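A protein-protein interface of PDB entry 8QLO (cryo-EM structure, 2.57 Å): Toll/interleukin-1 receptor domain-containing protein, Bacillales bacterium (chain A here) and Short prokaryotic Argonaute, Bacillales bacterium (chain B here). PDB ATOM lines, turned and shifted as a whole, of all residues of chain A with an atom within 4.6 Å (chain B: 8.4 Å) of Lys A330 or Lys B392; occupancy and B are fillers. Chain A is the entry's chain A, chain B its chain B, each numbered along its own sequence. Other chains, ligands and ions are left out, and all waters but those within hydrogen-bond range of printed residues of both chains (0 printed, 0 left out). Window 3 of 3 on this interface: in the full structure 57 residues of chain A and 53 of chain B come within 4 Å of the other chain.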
ATOM      1  N   TRP A 177       1.982 -26.496  -9.778  1.00  0.00           N
ATOM      2  CA  TRP A 177       0.865 -27.424  -9.859  1.00  0.00           C
ATOM      3  C   TRP A 177       0.887 -28.107 -11.218  1.00  0.00           C
ATOM      4  O   TRP A 177       0.894 -27.433 -12.253  1.00  0.00           O
ATOM      5  CB  TRP A 177      -0.460 -26.688  -9.675  1.00  0.00           C
ATOM      6  CG  TRP A 177      -0.729 -26.238  -8.283  1.00  0.00           C
ATOM      7  CD1 TRP A 177       0.137 -26.252  -7.234  1.00  0.00           C
ATOM      8  CD2 TRP A 177      -1.951 -25.686  -7.787  1.00  0.00           C
ATOM      9  NE1 TRP A 177      -0.471 -25.750  -6.112  1.00  0.00           N
ATOM     10  CE2 TRP A 177      -1.757 -25.397  -6.426  1.00  0.00           C
ATOM     11  CE3 TRP A 177      -3.194 -25.414  -8.363  1.00  0.00           C
ATOM     12  CZ2 TRP A 177      -2.756 -24.848  -5.631  1.00  0.00           C
ATOM     13  CZ3 TRP A 177      -4.185 -24.870  -7.573  1.00  0.00           C
ATOM     14  CH2 TRP A 177      -3.961 -24.592  -6.223  1.00  0.00           C
ATOM     15  N   ALA A 328       2.866 -33.445  -3.342  1.00  0.00           N
ATOM     16  CA  ALA A 328       1.642 -33.738  -2.616  1.00  0.00           C
ATOM     17  C   ALA A 328       0.499 -33.746  -3.617  1.00  0.00           C
ATOM     18  O   ALA A 328       0.647 -33.284  -4.748  1.00  0.00           O
ATOM     19  CB  ALA A 328       1.382 -32.721  -1.501  1.00  0.00           C
ATOM     20  N   GLY A 329      -0.645 -34.284  -3.204  1.00  0.00           N
ATOM     21  CA  GLY A 329      -1.817 -34.339  -4.047  1.00  0.00           C
ATOM     22  C   GLY A 329      -2.844 -33.290  -3.651  1.00  0.00           C
ATOM     23  O   GLY A 329      -2.875 -32.802  -2.523  1.00  0.00           O
ATOM     24  N   LYS A 330      -3.682 -32.914  -4.583  1.00  0.00           N
ATOM     25  CA  LYS A 330      -4.760 -32.004  -4.183  1.00  0.00           C
ATOM     26  C   LYS A 330      -5.870 -32.214  -5.184  1.00  0.00           C
ATOM     27  O   LYS A 330      -5.599 -32.140  -6.365  1.00  0.00           O
ATOM     28  CB  LYS A 330      -4.283 -30.563  -4.211  1.00  0.00           C
ATOM     29  CG  LYS A 330      -5.357 -29.555  -4.592  1.00  0.00           C
ATOM     30  CD  LYS A 330      -4.881 -28.128  -4.584  1.00  0.00           C
ATOM     31  CE  LYS A 330      -4.727 -27.581  -3.184  1.00  0.00           C
ATOM     32  NZ  LYS A 330      -6.010 -27.638  -2.450  1.00  0.00           N
ATOM     33  N   LEU A 331      -7.084 -32.505  -4.709  1.00  0.00           N
ATOM     34  CA  LEU A 331      -8.218 -32.794  -5.628  1.00  0.00           C
ATOM     35  C   LEU A 331      -9.040 -31.518  -5.833  1.00  0.00           C
ATOM     36  O   LEU A 331      -9.610 -31.354  -6.929  1.00  0.00           O
ATOM     37  CB  LEU A 331      -9.071 -33.916  -5.028  1.00  0.00           C
ATOM     38  CG  LEU A 331      -8.787 -35.319  -5.565  1.00  0.00           C
ATOM     39  CD1 LEU A 331      -7.350 -35.733  -5.289  1.00  0.00           C
ATOM     40  CD2 LEU A 331      -9.752 -36.331  -4.966  1.00  0.00           C
ATOM     41  N   TYR A 332      -9.006 -30.583  -4.895  1.00  0.00           N
ATOM     42  CA  TYR A 332      -9.733 -29.308  -5.133  1.00  0.00           C
ATOM     43  C   TYR A 332      -8.771 -28.172  -4.961  1.00  0.00           C
ATOM     44  O   TYR A 332      -8.002 -28.203  -3.996  1.00  0.00           O
ATOM     45  CB  TYR A 332     -10.870 -29.148  -4.128  1.00  0.00           C
ATOM     46  CG  TYR A 332     -11.921 -28.096  -4.433  1.00  0.00           C
ATOM     47  CD1 TYR A 332     -12.844 -28.286  -5.449  1.00  0.00           C
ATOM     48  CD2 TYR A 332     -11.978 -26.911  -3.715  1.00  0.00           C
ATOM     49  CE1 TYR A 332     -13.803 -27.333  -5.736  1.00  0.00           C
ATOM     50  CE2 TYR A 332     -12.929 -25.948  -3.994  1.00  0.00           C
ATOM     51  CZ  TYR A 332     -13.843 -26.160  -5.008  1.00  0.00           C
ATOM     52  OH  TYR A 332     -14.791 -25.226  -5.300  1.00  0.00           O
ATOM     53  N   PRO A 333      -8.776 -27.150  -5.832  1.00  0.00           N
ATOM     54  CA  PRO A 333      -9.886 -26.947  -6.735  1.00  0.00           C
ATOM     55  C   PRO A 333      -9.842 -27.810  -7.990  1.00  0.00           C
ATOM     56  O   PRO A 333     -10.865 -27.962  -8.605  1.00  0.00           O
ATOM     57  CB  PRO A 333      -9.654 -25.516  -7.189  1.00  0.00           C
ATOM     58  CG  PRO A 333      -8.167 -25.319  -7.108  1.00  0.00           C
ATOM     59  CD  PRO A 333      -7.738 -26.133  -5.912  1.00  0.00           C
ATOM     60  N   PHE A 334      -8.662 -28.316  -8.339  1.00  0.00           N
ATOM     61  CA  PHE A 334      -8.481 -29.125  -9.564  1.00  0.00           C
ATOM     62  C   PHE A 334      -7.502 -30.243  -9.251  1.00  0.00           C
ATOM     63  O   PHE A 334      -6.538 -30.016  -8.536  1.00  0.00           O
ATOM     64  CB  PHE A 334      -7.877 -28.290 -10.689  1.00  0.00           C
ATOM     65  CG  PHE A 334      -8.456 -26.917 -10.885  1.00  0.00           C
ATOM     66  CD1 PHE A 334      -9.773 -26.749 -11.275  1.00  0.00           C
ATOM     67  CD2 PHE A 334      -7.676 -25.793 -10.681  1.00  0.00           C
ATOM     68  CE1 PHE A 334     -10.301 -25.482 -11.452  1.00  0.00           C
ATOM     69  CE2 PHE A 334      -8.207 -24.527 -10.854  1.00  0.00           C
ATOM     70  CZ  PHE A 334      -9.518 -24.374 -11.240  1.00  0.00           C
ATOM     71  N   PRO A 335      -7.716 -31.451  -9.782  1.00  0.00           N
ATOM     72  CA  PRO A 335      -6.849 -32.538  -9.459  1.00  0.00           C
ATOM     73  C   PRO A 335      -5.450 -32.157  -9.915  1.00  0.00           C
ATOM     74  O   PRO A 335      -5.281 -31.995 -11.074  1.00  0.00           O
ATOM     75  CB  PRO A 335      -7.410 -33.588 -10.395  1.00  0.00           C
ATOM     76  CG  PRO A 335      -8.859 -33.267 -10.516  1.00  0.00           C
ATOM     77  CD  PRO A 335      -8.815 -31.773 -10.681  1.00  0.00           C
ATOM     78  N   VAL A 336      -4.497 -32.042  -9.003  1.00  0.00           N
ATOM     79  CA  VAL A 336      -3.127 -31.602  -9.372  1.00  0.00           C
ATOM     80  C   VAL A 336      -2.101 -32.224  -8.441  1.00  0.00           C
ATOM     81  O   VAL A 336      -2.454 -32.519  -7.320  1.00  0.00           O
ATOM     82  CB  VAL A 336      -2.995 -30.077  -9.303  1.00  0.00           C
ATOM     83  CG1 VAL A 336      -3.815 -29.349 -10.352  1.00  0.00           C
ATOM     84  CG2 VAL A 336      -3.276 -29.538  -7.915  1.00  0.00           C
ATOM     85  N   MET A 338       1.301 -31.271  -6.566  1.00  0.00           N
ATOM     86  CA  MET A 338       1.877 -29.946  -6.283  1.00  0.00           C
ATOM     87  C   MET A 338       3.324 -30.102  -5.901  1.00  0.00           C
ATOM     88  O   MET A 338       3.578 -30.348  -4.747  1.00  0.00           O
ATOM     89  CB  MET A 338       1.164 -29.338  -5.088  1.00  0.00           C
ATOM     90  CG  MET A 338      -0.305 -29.076  -5.342  1.00  0.00           C
ATOM     91  SD  MET A 338      -1.222 -28.570  -3.868  1.00  0.00           S
ATOM     92  CE  MET A 338      -0.311 -29.434  -2.593  1.00  0.00           C
ATOM     93  N   LYS B 364      -8.956 -22.751  11.833  1.00  0.00           N
ATOM     94  CA  LYS B 364     -10.363 -22.831  11.484  1.00  0.00           C
ATOM     95  C   LYS B 364     -11.232 -22.522  12.704  1.00  0.00           C
ATOM     96  O   LYS B 364     -10.740 -22.236  13.798  1.00  0.00           O
ATOM     97  CB  LYS B 364     -10.685 -24.211  10.915  1.00  0.00           C
ATOM     98  CG  LYS B 364     -11.196 -24.192   9.482  1.00  0.00           C
ATOM     99  CD  LYS B 364     -10.683 -25.385   8.695  1.00  0.00           C
ATOM    100  CE  LYS B 364     -10.902 -25.209   7.202  1.00  0.00           C
ATOM    101  NZ  LYS B 364     -10.370 -26.375   6.446  1.00  0.00           N
ATOM    102  N   ILE B 388      -6.634 -17.162   7.516  1.00  0.00           N
ATOM    103  CA  ILE B 388      -5.519 -16.723   6.690  1.00  0.00           C
ATOM    104  C   ILE B 388      -4.334 -17.627   6.988  1.00  0.00           C
ATOM    105  O   ILE B 388      -3.867 -17.688   8.131  1.00  0.00           O
ATOM    106  CB  ILE B 388      -5.167 -15.252   6.953  1.00  0.00           C
ATOM    107  CG1 ILE B 388      -6.310 -14.346   6.493  1.00  0.00           C
ATOM    108  CG2 ILE B 388      -3.871 -14.884   6.259  1.00  0.00           C
ATOM    109  CD1 ILE B 388      -6.047 -12.879   6.704  1.00  0.00           C
ATOM    110  N   THR B 389      -3.848 -18.323   5.965  1.00  0.00           N
ATOM    111  CA  THR B 389      -2.742 -19.254   6.130  1.00  0.00           C
ATOM    112  C   THR B 389      -1.629 -18.895   5.159  1.00  0.00           C
ATOM    113  O   THR B 389      -1.874 -18.330   4.093  1.00  0.00           O
ATOM    114  CB  THR B 389      -3.180 -20.705   5.907  1.00  0.00           C
ATOM    115  OG1 THR B 389      -4.174 -20.754   4.876  1.00  0.00           O
ATOM    116  CG2 THR B 389      -3.753 -21.290   7.186  1.00  0.00           C
ATOM    117  N   LYS B 390      -0.401 -19.223   5.541  1.00  0.00           N
ATOM    118  CA  LYS B 390       0.777 -18.977   4.720  1.00  0.00           C
ATOM    119  C   LYS B 390       1.482 -20.286   4.376  1.00  0.00           C
ATOM    120  O   LYS B 390       2.633 -20.305   3.935  1.00  0.00           O
ATOM    121  CB  LYS B 390       1.721 -17.997   5.418  1.00  0.00           C
ATOM    122  CG  LYS B 390       2.652 -18.618   6.449  1.00  0.00           C
ATOM    123  CD  LYS B 390       3.779 -17.665   6.814  1.00  0.00           C
ATOM    124  CE  LYS B 390       3.243 -16.308   7.236  1.00  0.00           C
ATOM    125  NZ  LYS B 390       4.240 -15.548   8.036  1.00  0.00           N
ATOM    126  N   THR B 391       0.769 -21.399   4.538  1.00  0.00           N
ATOM    127  CA  THR B 391       1.348 -22.726   4.378  1.00  0.00           C
ATOM    128  C   THR B 391       1.067 -23.377   3.029  1.00  0.00           C
ATOM    129  O   THR B 391       1.960 -24.056   2.504  1.00  0.00           O
ATOM    130  CB  THR B 391       0.850 -23.654   5.502  1.00  0.00           C
ATOM    131  OG1 THR B 391       1.583 -23.385   6.703  1.00  0.00           O
ATOM    132  CG2 THR B 391       1.017 -25.125   5.142  1.00  0.00           C
ATOM    133  N   LYS B 392      -0.104 -23.164   2.434  1.00  0.00           N
ATOM    134  CA  LYS B 392      -0.488 -23.905   1.238  1.00  0.00           C
ATOM    135  C   LYS B 392       0.509 -23.659   0.108  1.00  0.00           C
ATOM    136  O   LYS B 392       0.782 -22.501  -0.232  1.00  0.00           O
ATOM    137  CB  LYS B 392      -1.894 -23.511   0.796  1.00  0.00           C
ATOM    138  CG  LYS B 392      -2.954 -23.738   1.861  1.00  0.00           C
ATOM    139  CD  LYS B 392      -4.373 -23.791   1.296  1.00  0.00           C
ATOM    140  CE  LYS B 392      -4.702 -25.091   0.555  1.00  0.00           C
ATOM    141  NZ  LYS B 392      -3.822 -25.437  -0.596  1.00  0.00           N
ATOM    142  N   PRO B 393       1.066 -24.712  -0.493  1.00  0.00           N
ATOM    143  CA  PRO B 393       2.157 -24.529  -1.454  1.00  0.00           C
ATOM    144  C   PRO B 393       1.696 -24.298  -2.883  1.00  0.00           C
ATOM    145  O   PRO B 393       1.689 -25.228  -3.696  1.00  0.00           O
ATOM    146  CB  PRO B 393       2.943 -25.843  -1.330  1.00  0.00           C
ATOM    147  CG  PRO B 393       1.994 -26.826  -0.613  1.00  0.00           C
ATOM    148  CD  PRO B 393       0.680 -26.125  -0.406  1.00  0.00           C
ATOM    149  N   LEU B 394       1.406 -23.041  -3.231  1.00  0.00           N
ATOM    150  CA  LEU B 394       1.102 -22.718  -4.653  1.00  0.00           C
ATOM    151  C   LEU B 394       2.084 -21.626  -5.089  1.00  0.00           C
ATOM    152  O   LEU B 394       2.023 -20.534  -4.514  1.00  0.00           O
ATOM    153  CB  LEU B 394      -0.347 -22.242  -4.791  1.00  0.00           C
ATOM    154  CG  LEU B 394      -0.660 -21.494  -6.088  1.00  0.00           C
ATOM    155  CD1 LEU B 394      -0.414 -22.373  -7.306  1.00  0.00           C
ATOM    156  CD2 LEU B 394      -2.087 -20.973  -6.090  1.00  0.00           C
ATOM    157  N   LYS B 395       2.978 -21.915  -6.039  1.00  0.00           N
ATOM    158  CA  LYS B 395       4.008 -20.909  -6.417  1.00  0.00           C
ATOM    159  C   LYS B 395       3.845 -20.516  -7.888  1.00  0.00           C
ATOM    160  O   LYS B 395       3.856 -21.423  -8.739  1.00  0.00           O
ATOM    161  CB  LYS B 395       5.419 -21.448  -6.158  1.00  0.00           C
ATOM    162  CG  LYS B 395       5.936 -21.250  -4.740  1.00  0.00           C
ATOM    163  CD  LYS B 395       7.428 -21.467  -4.617  1.00  0.00           C
ATOM    164  CE  LYS B 395       7.976 -21.060  -3.265  1.00  0.00           C
ATOM    165  NZ  LYS B 395       9.453 -21.162  -3.221  1.00  0.00           N
ATOM    166  N   PHE B 411      -5.413 -15.433  -6.791  1.00  0.00           N
ATOM    167  CA  PHE B 411      -6.157 -16.537  -7.440  1.00  0.00           C
ATOM    168  C   PHE B 411      -7.444 -16.789  -6.659  1.00  0.00           C
ATOM    169  O   PHE B 411      -7.319 -17.209  -5.521  1.00  0.00           O
ATOM    170  CB  PHE B 411      -5.331 -17.816  -7.446  1.00  0.00           C
ATOM    171  CG  PHE B 411      -5.992 -18.940  -8.193  1.00  0.00           C
ATOM    172  CD1 PHE B 411      -6.629 -18.701  -9.397  1.00  0.00           C
ATOM    173  CD2 PHE B 411      -5.978 -20.229  -7.697  1.00  0.00           C
ATOM    174  CE1 PHE B 411      -7.252 -19.725 -10.085  1.00  0.00           C
ATOM    175  CE2 PHE B 411      -6.599 -21.253  -8.389  1.00  0.00           C
ATOM    176  CZ  PHE B 411      -7.234 -20.998  -9.578  1.00  0.00           C
ATOM    177  N   VAL B 413     -10.024 -19.128  -5.731  1.00  0.00           N
ATOM    178  CA  VAL B 413     -10.272 -20.566  -5.790  1.00  0.00           C
ATOM    179  C   VAL B 413     -11.762 -20.844  -5.949  1.00  0.00           C
ATOM    180  O   VAL B 413     -12.180 -21.622  -6.814  1.00  0.00           O
ATOM    181  CB  VAL B 413      -9.699 -21.257  -4.541  1.00  0.00           C
ATOM    182  CG1 VAL B 413     -10.340 -22.616  -4.344  1.00  0.00           C
ATOM    183  CG2 VAL B 413      -8.193 -21.384  -4.651  1.00  0.00           C
ATOM    184  N   SER B 417     -13.014 -18.701  -0.947  1.00  0.00           N
ATOM    185  CA  SER B 417     -11.566 -18.903  -0.666  1.00  0.00           C
ATOM    186  C   SER B 417     -10.735 -18.385  -1.844  1.00  0.00           C
ATOM    187  O   SER B 417     -11.233 -18.457  -2.985  1.00  0.00           O
ATOM    188  CB  SER B 417     -11.260 -20.348  -0.373  1.00  0.00           C
ATOM    189  OG  SER B 417     -11.379 -21.136  -1.545  1.00  0.00           O
ATOM    190  N   ALA B 418      -9.517 -17.896  -1.578  1.00  0.00           N
ATOM    191  CA  ALA B 418      -8.701 -17.305  -2.666  1.00  0.00           C
ATOM    192  C   ALA B 418      -7.235 -17.142  -2.255  1.00  0.00           C
ATOM    193  O   ALA B 418      -6.972 -16.989  -1.045  1.00  0.00           O
ATOM    194  CB  ALA B 418      -9.290 -15.976  -3.076  1.00  0.00           C
ATOM    195  N   PHE B 419      -6.320 -17.173  -3.230  1.00  0.00           N
ATOM    196  CA  PHE B 419      -4.905 -16.955  -2.977  1.00  0.00           C
ATOM    197  C   PHE B 419      -4.589 -15.491  -3.238  1.00  0.00           C
ATOM    198  O   PHE B 419      -5.000 -14.937  -4.261  1.00  0.00           O
ATOM    199  CB  PHE B 419      -4.029 -17.827  -3.879  1.00  0.00           C
ATOM    200  CG  PHE B 419      -3.919 -19.254  -3.436  1.00  0.00           C
ATOM    201  CD1 PHE B 419      -2.918 -19.645  -2.566  1.00  0.00           C
ATOM    202  CD2 PHE B 419      -4.799 -20.209  -3.910  1.00  0.00           C
ATOM    203  CE1 PHE B 419      -2.807 -20.958  -2.164  1.00  0.00           C
ATOM    204  CE2 PHE B 419      -4.693 -21.523  -3.510  1.00  0.00           C
ATOM    205  CZ  PHE B 419      -3.697 -21.898  -2.637  1.00  0.00           C
ATOM    206  N   PRO B 438       7.691 -15.550  -4.483  1.00  0.00           N
ATOM    207  CA  PRO B 438       6.605 -15.120  -3.592  1.00  0.00           C
ATOM    208  C   PRO B 438       5.701 -16.279  -3.205  1.00  0.00           C
ATOM    209  O   PRO B 438       5.180 -16.998  -4.060  1.00  0.00           O
ATOM    210  CB  PRO B 438       5.856 -14.079  -4.431  1.00  0.00           C
ATOM    211  CG  PRO B 438       6.846 -13.612  -5.427  1.00  0.00           C
ATOM    212  CD  PRO B 438       7.672 -14.812  -5.753  1.00  0.00           C
ATOM    213  N   ASN B 439       5.457 -16.423  -1.896  1.00  0.00           N
ATOM    214  CA  ASN B 439       4.512 -17.467  -1.413  1.00  0.00           C
ATOM    215  C   ASN B 439       3.160 -16.809  -1.115  1.00  0.00           C
ATOM    216  O   ASN B 439       3.081 -16.049  -0.131  1.00  0.00           O
ATOM    217  CB  ASN B 439       5.004 -18.169  -0.144  1.00  0.00           C
ATOM    218  CG  ASN B 439       6.422 -18.685  -0.243  1.00  0.00           C
ATOM    219  OD1 ASN B 439       7.088 -18.494  -1.256  1.00  0.00           O
ATOM    220  ND2 ASN B 439       6.896 -19.334   0.808  1.00  0.00           N
ATOM    221  N   PRO B 440       2.102 -17.062  -1.915  1.00  0.00           N
ATOM    222  CA  PRO B 440       0.781 -16.473  -1.680  1.00  0.00           C
ATOM    223  C   PRO B 440       0.082 -16.987  -0.415  1.00  0.00           C
ATOM    224  O   PRO B 440       0.222 -18.155  -0.102  1.00  0.00           O
ATOM    225  CB  PRO B 440      -0.042 -16.910  -2.901  1.00  0.00           C
ATOM    226  CG  PRO B 440       0.648 -18.165  -3.369  1.00  0.00           C
ATOM    227  CD  PRO B 440       2.117 -17.903  -3.110  1.00  0.00           C
ATOM    228  N   ILE B 441      -0.648 -16.107   0.273  1.00  0.00           N
ATOM    229  CA  ILE B 441      -1.394 -16.484   1.463  1.00  0.00           C
ATOM    230  C   ILE B 441      -2.801 -16.881   1.042  1.00  0.00           C
ATOM    231  O   ILE B 441      -3.424 -16.247   0.184  1.00  0.00           O
ATOM    232  CB  ILE B 441      -1.421 -15.352   2.511  1.00  0.00           C
ATOM    233  CG1 ILE B 441      -1.935 -14.054   1.891  1.00  0.00           C
ATOM    234  CG2 ILE B 441      -0.040 -15.140   3.099  1.00  0.00           C
ATOM    235  CD1 ILE B 441      -2.215 -12.971   2.902  1.00  0.00           C
ATOM    236  N   PHE B 442      -3.288 -17.959   1.641  1.00  0.00           N
ATOM    237  CA  PHE B 442      -4.624 -18.471   1.382  1.00  0.00           C
ATOM    238  C   PHE B 442      -5.610 -17.802   2.327  1.00  0.00           C
ATOM    239  O   PHE B 442      -5.448 -17.874   3.551  1.00  0.00           O
ATOM    240  CB  PHE B 442      -4.668 -19.988   1.561  1.00  0.00           C
ATOM    241  CG  PHE B 442      -5.894 -20.629   0.987  1.00  0.00           C
ATOM    242  CD1 PHE B 442      -6.195 -20.496  -0.355  1.00  0.00           C
ATOM    243  CD2 PHE B 442      -6.754 -21.352   1.791  1.00  0.00           C
ATOM    244  CE1 PHE B 442      -7.324 -21.080  -0.885  1.00  0.00           C
ATOM    245  CE2 PHE B 442      -7.882 -21.938   1.266  1.00  0.00           C
ATOM    246  CZ  PHE B 442      -8.166 -21.803  -0.074  1.00  0.00           C
ATOM    247  N   ILE B 443      -6.617 -17.147   1.758  1.00  0.00           N
ATOM    248  CA  ILE B 443      -7.677 -16.494   2.514  1.00  0.00           C
ATOM    249  C   ILE B 443      -8.961 -17.270   2.261  1.00  0.00           C
ATOM    250  O   ILE B 443      -9.366 -17.448   1.107  1.00  0.00           O
ATOM    251  CB  ILE B 443      -7.840 -15.014   2.112  1.00  0.00           C
ATOM    252  CG1 ILE B 443      -6.943 -14.101   2.953  1.00  0.00           C
ATOM    253  CG2 ILE B 443      -9.282 -14.563   2.259  1.00  0.00           C
ATOM    254  CD1 ILE B 443      -5.479 -14.428   2.903  1.00  0.00           C
ATOM    255  N   GLU B 444      -9.593 -17.744   3.332  1.00  0.00           N
ATOM    256  CA  GLU B 444     -10.843 -18.484   3.219  1.00  0.00           C
ATOM    257  C   GLU B 444     -11.883 -17.852   4.127  1.00  0.00           C
ATOM    258  O   GLU B 444     -11.601 -17.568   5.294  1.00  0.00           O
ATOM    259  CB  GLU B 444     -10.658 -19.962   3.584  1.00  0.00           C
ATOM    260  CG  GLU B 444      -9.586 -20.209   4.625  1.00  0.00           C
ATOM    261  CD  GLU B 444      -9.195 -21.670   4.745  1.00  0.00           C
ATOM    262  OE1 GLU B 444      -7.980 -21.963   4.726  1.00  0.00           O
ATOM    263  OE2 GLU B 444     -10.098 -22.524   4.864  1.00  0.00           O
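The backbone carbonyl oxygen (O) of Pro B393 lies within hydrogen-bond range of the indole nitrogen (NE1) of Trp A177, at 3.3 Å.
Of the 11 printed residues of chain A, 3 touch a printed residue of chain B.
Hydrophobic or aromatic side chains of chain A within 4 Å of the printed part of chain B: Trp A177 and Phe A334.
Among the printed residues, 4 pairs touch across the chains.
Trp A177 touches Leu B394.
Lys A330 touches Lys B392.
Phe B411 touches Phe A334 (CZ to CE2, 3.9 Å).
Lys B392 touches just one residue of chain A: Lys A330 (3.5 Å).
Gly A329 touches none of the printed residues of chain B.
Of the printed residues of chain B, Trp A177 touches Pro B393 (3.3 Å) and Leu B394 (3.4 Å).
Of the printed residues of chain B, Phe A334 touches Phe B411 (3.9 Å).
Printed residues of chain A within 4 Å of Pro B393: Trp A177.
Of the printed residues of chain A, Phe B411 touches Phe A334.
Pro A335 touches none of the printed residues of chain B.
The nearest residue of chain B that does not touch Lys A330 is Phe B419 (5.8 Å).
The nearest printed residue of chain B that does not touch Phe A334 is Val B413 (5.9 Å).
The backbone NH (N) of Phe B419 sits at hydrogen-bond distance from the backbone carbonyl oxygen (O) of Phe B411, 2.5 Å away.
The indole nitrogen (NE1) of Trp A177 sits close to the side-chain sulfur (SD) of Met A338 (3.7 Å).
O of Tyr A332 is in hydrogen-bond range of NZ of Lys A330.
The backbone carbonyl oxygen of Lys A330 sits at hydrogen-bond distance from the backbone NH of Val A336 (2.9 Å).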
